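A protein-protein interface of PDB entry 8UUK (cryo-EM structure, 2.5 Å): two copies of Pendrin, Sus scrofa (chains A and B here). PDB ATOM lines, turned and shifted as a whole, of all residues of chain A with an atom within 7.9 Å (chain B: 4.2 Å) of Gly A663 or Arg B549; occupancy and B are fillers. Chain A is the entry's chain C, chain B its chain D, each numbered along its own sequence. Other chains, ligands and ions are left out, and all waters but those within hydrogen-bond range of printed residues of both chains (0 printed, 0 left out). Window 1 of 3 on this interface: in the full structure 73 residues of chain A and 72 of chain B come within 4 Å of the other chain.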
ATOM      1  N   LEU A 548      25.183  43.694   7.232  1.00  0.00           N
ATOM      2  CA  LEU A 548      26.327  43.205   7.989  1.00  0.00           C
ATOM      3  C   LEU A 548      26.268  41.688   8.051  1.00  0.00           C
ATOM      4  O   LEU A 548      25.235  41.117   8.412  1.00  0.00           O
ATOM      5  CB  LEU A 548      26.355  43.791   9.401  1.00  0.00           C
ATOM      6  CG  LEU A 548      27.476  43.245  10.289  1.00  0.00           C
ATOM      7  CD1 LEU A 548      28.775  43.984  10.037  1.00  0.00           C
ATOM      8  CD2 LEU A 548      27.094  43.316  11.752  1.00  0.00           C
ATOM      9  N   ARG A 549      27.373  41.041   7.699  1.00  0.00           N
ATOM     10  CA  ARG A 549      27.512  39.599   7.831  1.00  0.00           C
ATOM     11  C   ARG A 549      28.467  39.309   8.980  1.00  0.00           C
ATOM     12  O   ARG A 549      29.630  39.721   8.943  1.00  0.00           O
ATOM     13  CB  ARG A 549      28.024  38.976   6.533  1.00  0.00           C
ATOM     14  CG  ARG A 549      28.634  37.603   6.712  1.00  0.00           C
ATOM     15  CD  ARG A 549      28.537  36.788   5.439  1.00  0.00           C
ATOM     16  NE  ARG A 549      28.774  35.371   5.685  1.00  0.00           N
ATOM     17  CZ  ARG A 549      27.870  34.419   5.508  1.00  0.00           C
ATOM     18  NH1 ARG A 549      26.650  34.696   5.080  1.00  0.00           N
ATOM     19  NH2 ARG A 549      28.199  33.157   5.762  1.00  0.00           N
ATOM     20  N   PHE A 550      27.974  38.615   9.998  1.00  0.00           N
ATOM     21  CA  PHE A 550      28.775  38.212  11.151  1.00  0.00           C
ATOM     22  C   PHE A 550      29.017  36.714  11.019  1.00  0.00           C
ATOM     23  O   PHE A 550      28.159  35.903  11.380  1.00  0.00           O
ATOM     24  CB  PHE A 550      28.071  38.564  12.458  1.00  0.00           C
ATOM     25  CG  PHE A 550      28.974  38.563  13.654  1.00  0.00           C
ATOM     26  CD1 PHE A 550      29.946  39.535  13.805  1.00  0.00           C
ATOM     27  CD2 PHE A 550      28.848  37.592  14.634  1.00  0.00           C
ATOM     28  CE1 PHE A 550      30.777  39.538  14.905  1.00  0.00           C
ATOM     29  CE2 PHE A 550      29.675  37.592  15.736  1.00  0.00           C
ATOM     30  CZ  PHE A 550      30.640  38.566  15.872  1.00  0.00           C
ATOM     31  N   SER A 551      30.188  36.350  10.502  1.00  0.00           N
ATOM     32  CA  SER A 551      30.472  34.966  10.129  1.00  0.00           C
ATOM     33  C   SER A 551      30.941  34.154  11.339  1.00  0.00           C
ATOM     34  O   SER A 551      32.076  33.686  11.411  1.00  0.00           O
ATOM     35  CB  SER A 551      31.498  34.925   9.004  1.00  0.00           C
ATOM     36  OG  SER A 551      31.006  35.571   7.845  1.00  0.00           O
ATOM     37  N   SER A 552      30.026  33.983  12.291  1.00  0.00           N
ATOM     38  CA  SER A 552      30.289  33.185  13.482  1.00  0.00           C
ATOM     39  C   SER A 552      29.006  32.937  14.260  1.00  0.00           C
ATOM     40  O   SER A 552      28.050  33.714  14.150  1.00  0.00           O
ATOM     41  CB  SER A 552      31.305  33.877  14.390  1.00  0.00           C
ATOM     42  OG  SER A 552      32.151  32.936  15.024  1.00  0.00           O
ATOM     43  N   LEU A 660      20.974  41.906   8.920  1.00  0.00           N
ATOM     44  CA  LEU A 660      22.003  41.066   9.520  1.00  0.00           C
ATOM     45  C   LEU A 660      22.050  39.743   8.765  1.00  0.00           C
ATOM     46  O   LEU A 660      21.129  38.928   8.871  1.00  0.00           O
ATOM     47  CB  LEU A 660      21.725  40.845  11.005  1.00  0.00           C
ATOM     48  CG  LEU A 660      22.062  42.017  11.926  1.00  0.00           C
ATOM     49  CD1 LEU A 660      21.793  41.659  13.375  1.00  0.00           C
ATOM     50  CD2 LEU A 660      23.506  42.443  11.743  1.00  0.00           C
ATOM     51  N   ASP A 661      23.118  39.536   8.001  1.00  0.00           N
ATOM     52  CA  ASP A 661      23.325  38.283   7.278  1.00  0.00           C
ATOM     53  C   ASP A 661      23.852  37.254   8.268  1.00  0.00           C
ATOM     54  O   ASP A 661      25.027  37.274   8.641  1.00  0.00           O
ATOM     55  CB  ASP A 661      24.288  38.481   6.114  1.00  0.00           C
ATOM     56  CG  ASP A 661      24.457  37.227   5.278  1.00  0.00           C
ATOM     57  OD1 ASP A 661      23.624  36.307   5.405  1.00  0.00           O
ATOM     58  OD2 ASP A 661      25.425  37.162   4.492  1.00  0.00           O
ATOM     59  N   CYS A 662      22.980  36.349   8.699  1.00  0.00           N
ATOM     60  CA  CYS A 662      23.300  35.364   9.725  1.00  0.00           C
ATOM     61  C   CYS A 662      23.416  33.961   9.138  1.00  0.00           C
ATOM     62  O   CYS A 662      23.026  32.974   9.764  1.00  0.00           O
ATOM     63  CB  CYS A 662      22.260  35.396  10.838  1.00  0.00           C
ATOM     64  SG  CYS A 662      21.889  37.047  11.463  1.00  0.00           S
ATOM     65  N   GLY A 663      23.953  33.861   7.922  1.00  0.00           N
ATOM     66  CA  GLY A 663      24.129  32.555   7.308  1.00  0.00           C
ATOM     67  C   GLY A 663      25.129  31.690   8.048  1.00  0.00           C
ATOM     68  O   GLY A 663      24.974  30.470   8.124  1.00  0.00           O
ATOM     69  N   ALA A 664      26.169  32.307   8.603  1.00  0.00           N
ATOM     70  CA  ALA A 664      27.229  31.585   9.289  1.00  0.00           C
ATOM     71  C   ALA A 664      27.029  31.507  10.795  1.00  0.00           C
ATOM     72  O   ALA A 664      27.920  31.021  11.497  1.00  0.00           O
ATOM     73  CB  ALA A 664      28.585  32.221   8.982  1.00  0.00           C
ATOM     74  N   VAL A 665      25.893  31.973  11.309  1.00  0.00           N
ATOM     75  CA  VAL A 665      25.610  31.863  12.737  1.00  0.00           C
ATOM     76  C   VAL A 665      25.240  30.412  13.027  1.00  0.00           C
ATOM     77  O   VAL A 665      24.113  29.983  12.768  1.00  0.00           O
ATOM     78  CB  VAL A 665      24.498  32.826  13.167  1.00  0.00           C
ATOM     79  CG1 VAL A 665      24.111  32.581  14.615  1.00  0.00           C
ATOM     80  CG2 VAL A 665      24.950  34.262  12.976  1.00  0.00           C
ATOM     81  N   SER A 666      26.195  29.650  13.561  1.00  0.00           N
ATOM     82  CA  SER A 666      26.004  28.216  13.743  1.00  0.00           C
ATOM     83  C   SER A 666      25.083  27.923  14.922  1.00  0.00           C
ATOM     84  O   SER A 666      24.021  27.314  14.757  1.00  0.00           O
ATOM     85  CB  SER A 666      27.359  27.531  13.933  1.00  0.00           C
ATOM     86  OG  SER A 666      28.276  27.940  12.935  1.00  0.00           O
ATOM     87  N   PHE A 692      16.842  40.067   9.924  1.00  0.00           N
ATOM     88  CA  PHE A 692      17.741  38.925   9.946  1.00  0.00           C
ATOM     89  C   PHE A 692      17.502  38.073   8.709  1.00  0.00           C
ATOM     90  O   PHE A 692      16.356  37.800   8.345  1.00  0.00           O
ATOM     91  CB  PHE A 692      17.535  38.090  11.211  1.00  0.00           C
ATOM     92  CG  PHE A 692      17.725  38.862  12.483  1.00  0.00           C
ATOM     93  CD1 PHE A 692      16.691  39.611  13.017  1.00  0.00           C
ATOM     94  CD2 PHE A 692      18.938  38.839  13.148  1.00  0.00           C
ATOM     95  CE1 PHE A 692      16.865  40.322  14.185  1.00  0.00           C
ATOM     96  CE2 PHE A 692      19.117  39.547  14.317  1.00  0.00           C
ATOM     97  CZ  PHE A 692      18.079  40.290  14.836  1.00  0.00           C
ATOM     98  N   ALA A 693      18.587  37.664   8.059  1.00  0.00           N
ATOM     99  CA  ALA A 693      18.489  36.893   6.831  1.00  0.00           C
ATOM    100  C   ALA A 693      19.439  35.708   6.891  1.00  0.00           C
ATOM    101  O   ALA A 693      20.454  35.740   7.593  1.00  0.00           O
ATOM    102  CB  ALA A 693      18.793  37.754   5.603  1.00  0.00           C
ATOM    103  N   SER A 694      19.087  34.657   6.153  1.00  0.00           N
ATOM    104  CA  SER A 694      19.884  33.438   6.024  1.00  0.00           C
ATOM    105  C   SER A 694      20.056  32.704   7.349  1.00  0.00           C
ATOM    106  O   SER A 694      20.974  31.892   7.495  1.00  0.00           O
ATOM    107  CB  SER A 694      21.253  33.732   5.401  1.00  0.00           C
ATOM    108  OG  SER A 694      21.119  34.169   4.060  1.00  0.00           O
ATOM    109  N   LEU A 695      19.188  32.963   8.322  1.00  0.00           N
ATOM    110  CA  LEU A 695      19.251  32.234   9.580  1.00  0.00           C
ATOM    111  C   LEU A 695      18.786  30.798   9.390  1.00  0.00           C
ATOM    112  O   LEU A 695      17.787  30.534   8.717  1.00  0.00           O
ATOM    113  CB  LEU A 695      18.399  32.921  10.645  1.00  0.00           C
ATOM    114  CG  LEU A 695      19.176  33.809  11.614  1.00  0.00           C
ATOM    115  CD1 LEU A 695      18.240  34.675  12.424  1.00  0.00           C
ATOM    116  CD2 LEU A 695      20.046  32.967  12.521  1.00  0.00           C
ATOM    117  N   GLN A 696      19.517  29.868   9.995  1.00  0.00           N
ATOM    118  CA  GLN A 696      19.176  28.461   9.892  1.00  0.00           C
ATOM    119  C   GLN A 696      17.930  28.153  10.717  1.00  0.00           C
ATOM    120  O   GLN A 696      17.535  28.912  11.605  1.00  0.00           O
ATOM    121  CB  GLN A 696      20.344  27.593  10.352  1.00  0.00           C
ATOM    122  CG  GLN A 696      21.446  27.446   9.318  1.00  0.00           C
ATOM    123  CD  GLN A 696      20.913  27.093   7.947  1.00  0.00           C
ATOM    124  OE1 GLN A 696      20.921  27.919   7.035  1.00  0.00           O
ATOM    125  NE2 GLN A 696      20.446  25.861   7.792  1.00  0.00           N
ATOM    126  N   ASP A 697      17.301  27.019  10.399  1.00  0.00           N
ATOM    127  CA  ASP A 697      16.071  26.638  11.085  1.00  0.00           C
ATOM    128  C   ASP A 697      16.310  26.403  12.571  1.00  0.00           C
ATOM    129  O   ASP A 697      15.530  26.866  13.411  1.00  0.00           O
ATOM    130  CB  ASP A 697      15.475  25.389  10.437  1.00  0.00           C
ATOM    131  CG  ASP A 697      14.709  25.700   9.169  1.00  0.00           C
ATOM    132  OD1 ASP A 697      14.171  26.821   9.059  1.00  0.00           O
ATOM    133  OD2 ASP A 697      14.643  24.823   8.284  1.00  0.00           O
ATOM    134  N   HIS A 698      17.386  25.691  12.916  1.00  0.00           N
ATOM    135  CA  HIS A 698      17.642  25.377  14.318  1.00  0.00           C
ATOM    136  C   HIS A 698      17.972  26.625  15.128  1.00  0.00           C
ATOM    137  O   HIS A 698      17.612  26.708  16.308  1.00  0.00           O
ATOM    138  CB  HIS A 698      18.765  24.343  14.428  1.00  0.00           C
ATOM    139  CG  HIS A 698      20.103  24.847  13.985  1.00  0.00           C
ATOM    140  ND1 HIS A 698      20.473  24.909  12.660  1.00  0.00           N
ATOM    141  CD2 HIS A 698      21.163  25.304  14.694  1.00  0.00           C
ATOM    142  CE1 HIS A 698      21.702  25.386  12.569  1.00  0.00           C
ATOM    143  NE2 HIS A 698      22.142  25.635  13.790  1.00  0.00           N
ATOM    144  N   VAL A 699      18.638  27.607  14.521  1.00  0.00           N
ATOM    145  CA  VAL A 699      18.895  28.858  15.225  1.00  0.00           C
ATOM    146  C   VAL A 699      17.590  29.601  15.482  1.00  0.00           C
ATOM    147  O   VAL A 699      17.418  30.241  16.526  1.00  0.00           O
ATOM    148  CB  VAL A 699      19.899  29.720  14.443  1.00  0.00           C
ATOM    149  CG1 VAL A 699      20.462  30.806  15.339  1.00  0.00           C
ATOM    150  CG2 VAL A 699      21.014  28.859  13.887  1.00  0.00           C
ATOM    151  N   LEU A 720      14.757  34.720   4.061  1.00  0.00           N
ATOM    152  CA  LEU A 720      15.472  33.498   3.709  1.00  0.00           C
ATOM    153  C   LEU A 720      16.915  33.781   3.312  1.00  0.00           C
ATOM    154  O   LEU A 720      17.828  33.056   3.720  1.00  0.00           O
ATOM    155  CB  LEU A 720      14.745  32.772   2.579  1.00  0.00           C
ATOM    156  CG  LEU A 720      13.262  32.469   2.782  1.00  0.00           C
ATOM    157  CD1 LEU A 720      12.785  31.519   1.706  1.00  0.00           C
ATOM    158  CD2 LEU A 720      13.003  31.891   4.161  1.00  0.00           C
ATOM    159  N   VAL A 722      19.827  37.199   1.952  1.00  0.00           N
ATOM    160  CA  VAL A 722      19.928  38.644   1.812  1.00  0.00           C
ATOM    161  C   VAL A 722      19.736  38.973   0.341  1.00  0.00           C
ATOM    162  O   VAL A 722      20.668  39.401  -0.346  1.00  0.00           O
ATOM    163  CB  VAL A 722      21.281  39.177   2.318  1.00  0.00           C
ATOM    164  CG1 VAL A 722      21.230  40.688   2.465  1.00  0.00           C
ATOM    165  CG2 VAL A 722      21.659  38.517   3.625  1.00  0.00           C
ATOM    166  N   SER B 517      24.724  21.278  13.711  1.00  0.00           N
ATOM    167  CA  SER B 517      23.553  20.781  13.008  1.00  0.00           C
ATOM    168  C   SER B 517      23.887  20.603  11.534  1.00  0.00           C
ATOM    169  O   SER B 517      24.286  21.557  10.860  1.00  0.00           O
ATOM    170  CB  SER B 517      22.380  21.745  13.176  1.00  0.00           C
ATOM    171  OG  SER B 517      21.335  21.439  12.270  1.00  0.00           O
ATOM    172  N   TRP B 518      23.730  19.382  11.037  1.00  0.00           N
ATOM    173  CA  TRP B 518      24.004  19.069   9.644  1.00  0.00           C
ATOM    174  C   TRP B 518      22.759  18.465   9.017  1.00  0.00           C
ATOM    175  O   TRP B 518      22.063  17.664   9.648  1.00  0.00           O
ATOM    176  CB  TRP B 518      25.187  18.108   9.510  1.00  0.00           C
ATOM    177  CG  TRP B 518      24.987  16.812  10.221  1.00  0.00           C
ATOM    178  CD1 TRP B 518      25.235  16.552  11.535  1.00  0.00           C
ATOM    179  CD2 TRP B 518      24.502  15.591   9.654  1.00  0.00           C
ATOM    180  NE1 TRP B 518      24.930  15.244  11.824  1.00  0.00           N
ATOM    181  CE2 TRP B 518      24.479  14.633  10.684  1.00  0.00           C
ATOM    182  CE3 TRP B 518      24.083  15.215   8.374  1.00  0.00           C
ATOM    183  CZ2 TRP B 518      24.054  13.324  10.476  1.00  0.00           C
ATOM    184  CZ3 TRP B 518      23.662  13.918   8.170  1.00  0.00           C
ATOM    185  CH2 TRP B 518      23.651  12.987   9.215  1.00  0.00           C
ATOM    186  N   ASN B 519      22.479  18.855   7.779  1.00  0.00           N
ATOM    187  CA  ASN B 519      21.259  18.453   7.099  1.00  0.00           C
ATOM    188  C   ASN B 519      21.570  18.006   5.679  1.00  0.00           C
ATOM    189  O   ASN B 519      22.535  18.462   5.063  1.00  0.00           O
ATOM    190  CB  ASN B 519      20.242  19.599   7.062  1.00  0.00           C
ATOM    191  CG  ASN B 519      19.604  19.855   8.409  1.00  0.00           C
ATOM    192  OD1 ASN B 519      19.160  18.927   9.085  1.00  0.00           O
ATOM    193  ND2 ASN B 519      19.553  21.119   8.809  1.00  0.00           N
ATOM    194  N   LEU B 521      20.157  18.544   2.255  1.00  0.00           N
ATOM    195  CA  LEU B 521      19.279  19.561   1.695  1.00  0.00           C
ATOM    196  C   LEU B 521      18.679  19.114   0.370  1.00  0.00           C
ATOM    197  O   LEU B 521      19.311  18.394  -0.406  1.00  0.00           O
ATOM    198  CB  LEU B 521      20.036  20.874   1.498  1.00  0.00           C
ATOM    199  CG  LEU B 521      20.755  21.439   2.721  1.00  0.00           C
ATOM    200  CD1 LEU B 521      21.471  22.724   2.359  1.00  0.00           C
ATOM    201  CD2 LEU B 521      19.773  21.668   3.854  1.00  0.00           C
ATOM    202  N   LEU B 548      24.786  18.454   1.263  1.00  0.00           N
ATOM    203  CA  LEU B 548      25.027  18.405   2.698  1.00  0.00           C
ATOM    204  C   LEU B 548      25.428  19.788   3.182  1.00  0.00           C
ATOM    205  O   LEU B 548      26.330  20.411   2.613  1.00  0.00           O
ATOM    206  CB  LEU B 548      26.113  17.386   3.047  1.00  0.00           C
ATOM    207  CG  LEU B 548      26.490  17.349   4.530  1.00  0.00           C
ATOM    208  CD1 LEU B 548      25.528  16.475   5.312  1.00  0.00           C
ATOM    209  CD2 LEU B 548      27.915  16.875   4.717  1.00  0.00           C
ATOM    210  N   ARG B 549      24.761  20.264   4.226  1.00  0.00           N
ATOM    211  CA  ARG B 549      25.117  21.512   4.882  1.00  0.00           C
ATOM    212  C   ARG B 549      25.739  21.189   6.233  1.00  0.00           C
ATOM    213  O   ARG B 549      25.082  20.602   7.097  1.00  0.00           O
ATOM    214  CB  ARG B 549      23.895  22.412   5.050  1.00  0.00           C
ATOM    215  CG  ARG B 549      24.064  23.482   6.107  1.00  0.00           C
ATOM    216  CD  ARG B 549      23.183  24.680   5.825  1.00  0.00           C
ATOM    217  NE  ARG B 549      23.589  25.844   6.602  1.00  0.00           N
ATOM    218  CZ  ARG B 549      24.055  26.969   6.078  1.00  0.00           C
ATOM    219  NH1 ARG B 549      24.187  27.120   4.772  1.00  0.00           N
ATOM    220  NH2 ARG B 549      24.395  27.968   6.886  1.00  0.00           N
ATOM    221  N   PHE B 550      27.003  21.557   6.406  1.00  0.00           N
ATOM    222  CA  PHE B 550      27.722  21.370   7.663  1.00  0.00           C
ATOM    223  C   PHE B 550      27.813  22.738   8.327  1.00  0.00           C
ATOM    224  O   PHE B 550      28.686  23.544   7.992  1.00  0.00           O
ATOM    225  CB  PHE B 550      29.098  20.760   7.421  1.00  0.00           C
ATOM    226  CG  PHE B 550      29.724  20.165   8.648  1.00  0.00           C
ATOM    227  CD1 PHE B 550      29.205  19.015   9.216  1.00  0.00           C
ATOM    228  CD2 PHE B 550      30.836  20.749   9.229  1.00  0.00           C
ATOM    229  CE1 PHE B 550      29.779  18.464  10.342  1.00  0.00           C
ATOM    230  CE2 PHE B 550      31.412  20.203  10.355  1.00  0.00           C
ATOM    231  CZ  PHE B 550      30.884  19.058  10.911  1.00  0.00           C
ATOM    232  N   SER B 551      26.913  22.997   9.271  1.00  0.00           N
ATOM    233  CA  SER B 551      26.755  24.332   9.845  1.00  0.00           C
ATOM    234  C   SER B 551      27.759  24.570  10.973  1.00  0.00           C
ATOM    235  O   SER B 551      27.406  24.737  12.139  1.00  0.00           O
ATOM    236  CB  SER B 551      25.324  24.530  10.328  1.00  0.00           C
ATOM    237  OG  SER B 551      24.406  24.435   9.254  1.00  0.00           O
ATOM    238  N   ASP B 661      27.270  22.442   1.156  1.00  0.00           N
ATOM    239  CA  ASP B 661      26.821  23.792   1.490  1.00  0.00           C
ATOM    240  C   ASP B 661      27.659  24.287   2.660  1.00  0.00           C
ATOM    241  O   ASP B 661      27.457  23.875   3.805  1.00  0.00           O
ATOM    242  CB  ASP B 661      25.334  23.801   1.824  1.00  0.00           C
ATOM    243  CG  ASP B 661      24.804  25.197   2.085  1.00  0.00           C
ATOM    244  OD1 ASP B 661      25.490  26.175   1.721  1.00  0.00           O
ATOM    245  OD2 ASP B 661      23.699  25.319   2.653  1.00  0.00           O
ATOM    246  N   GLY B 663      28.025  27.511   3.785  1.00  0.00           N
ATOM    247  CA  GLY B 663      27.697  28.876   4.156  1.00  0.00           C
ATOM    248  C   GLY B 663      28.073  29.200   5.588  1.00  0.00           C
ATOM    249  O   GLY B 663      28.475  30.324   5.896  1.00  0.00           O
ATOM    250  N   ALA B 664      27.949  28.222   6.481  1.00  0.00           N
ATOM    251  CA  ALA B 664      28.219  28.419   7.897  1.00  0.00           C
ATOM    252  C   ALA B 664      29.631  28.020   8.302  1.00  0.00           C
ATOM    253  O   ALA B 664      29.942  28.034   9.495  1.00  0.00           O
ATOM    254  CB  ALA B 664      27.204  27.647   8.740  1.00  0.00           C
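Arg A549 touches Gly B663, and with the chains exchanged Gly A663 touches Arg B549.
Gly A663 touches Ala B664, and with the chains exchanged Ala A664 touches Gly B663.
Ala A664 touches its own counterpart, Ala B664.
7 positions are printed for both chains.
Of the 9 pairs that touch across the chains among the printed residues, 5 have their exchanged pair printed and touching as well.
Printed residues of chain A that touch a printed residue of chain B: Arg A549, Gly A663, Ala A664, Ser A666, Gln A696 and His A698.
Of the 11 printed residues of chain B, 5 touch a printed residue of chain A.
Hydrophobic or aromatic side chains of chain B within 4 Å of the printed part of chain A: Ala B664.
Among the printed residues, pairs that only touch across the chains: His A698 with Ser B517 (3.6 Å), Ala A664 with Ala B664 (3.6 Å), Ala A664 with Gly B663 (3.6 Å), Gly A663 with Ala B664 (3.6 Å) and Ser A666 with Ala B664 (3.8 Å).
The guanidinium group (NH1) of Arg B549 is in salt-bridge range of the side-chain carboxylate (OD2) of Asp B661 (2.8 Å).
The guanidinium group of Arg B549 is in hydrogen-bond range of the side-chain hydroxyl of Ser B551 (3.1 Å).
O of Ser A666 sits at hydrogen-bond distance from NE2 of His A698, 2.7 Å away.
The side-chain hydroxyl (OG) of Ser A666 lies within hydrogen-bond range of the backbone carbonyl oxygen (O) of Ala A664, at 3.4 Å.
The side-chain hydroxyl of Ser A551 is in hydrogen-bond range of the guanidinium group of Arg A549 (3.1 Å).
The guanidinium group (NH1) of Arg A549 lies within salt-bridge range of the side-chain carboxylate (OD2) of Asp A661.
Gly A663 touches just these residues of chain B: Arg B549 and Ala B664.
Of chain A, only Gly A663 (2.9 Å) and Gln A696 (3.2 Å) come within 4 Å of Arg B549.
Printed residues of chain A within 4 Å of Ala B664: Gly A663, Ala A664 and Ser A666.
Printed residues of chain A within 4 Å of Ser B551: Ser A666.
Of the printed residues of chain A, Ser B517 touches His A698 (3.6 Å).
Of the printed residues of chain B, Gln A696 touches Arg B549.
The nearest printed residue of chain B that does not touch Gly A663 is Gly B663 (4.2 Å).
OG of Ser A666 lies close to O of Ser B551.
The guanidinium group of Arg B549 lies within hydrogen-bond range of the backbone carbonyl oxygen of Gly A663 (2.9 Å).
NE2 of Gln A696 lies close to NE of Arg B549, 3.4 Å away.
O of Gly B663 sits at hydrogen-bond distance from NH2 of Arg A549.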
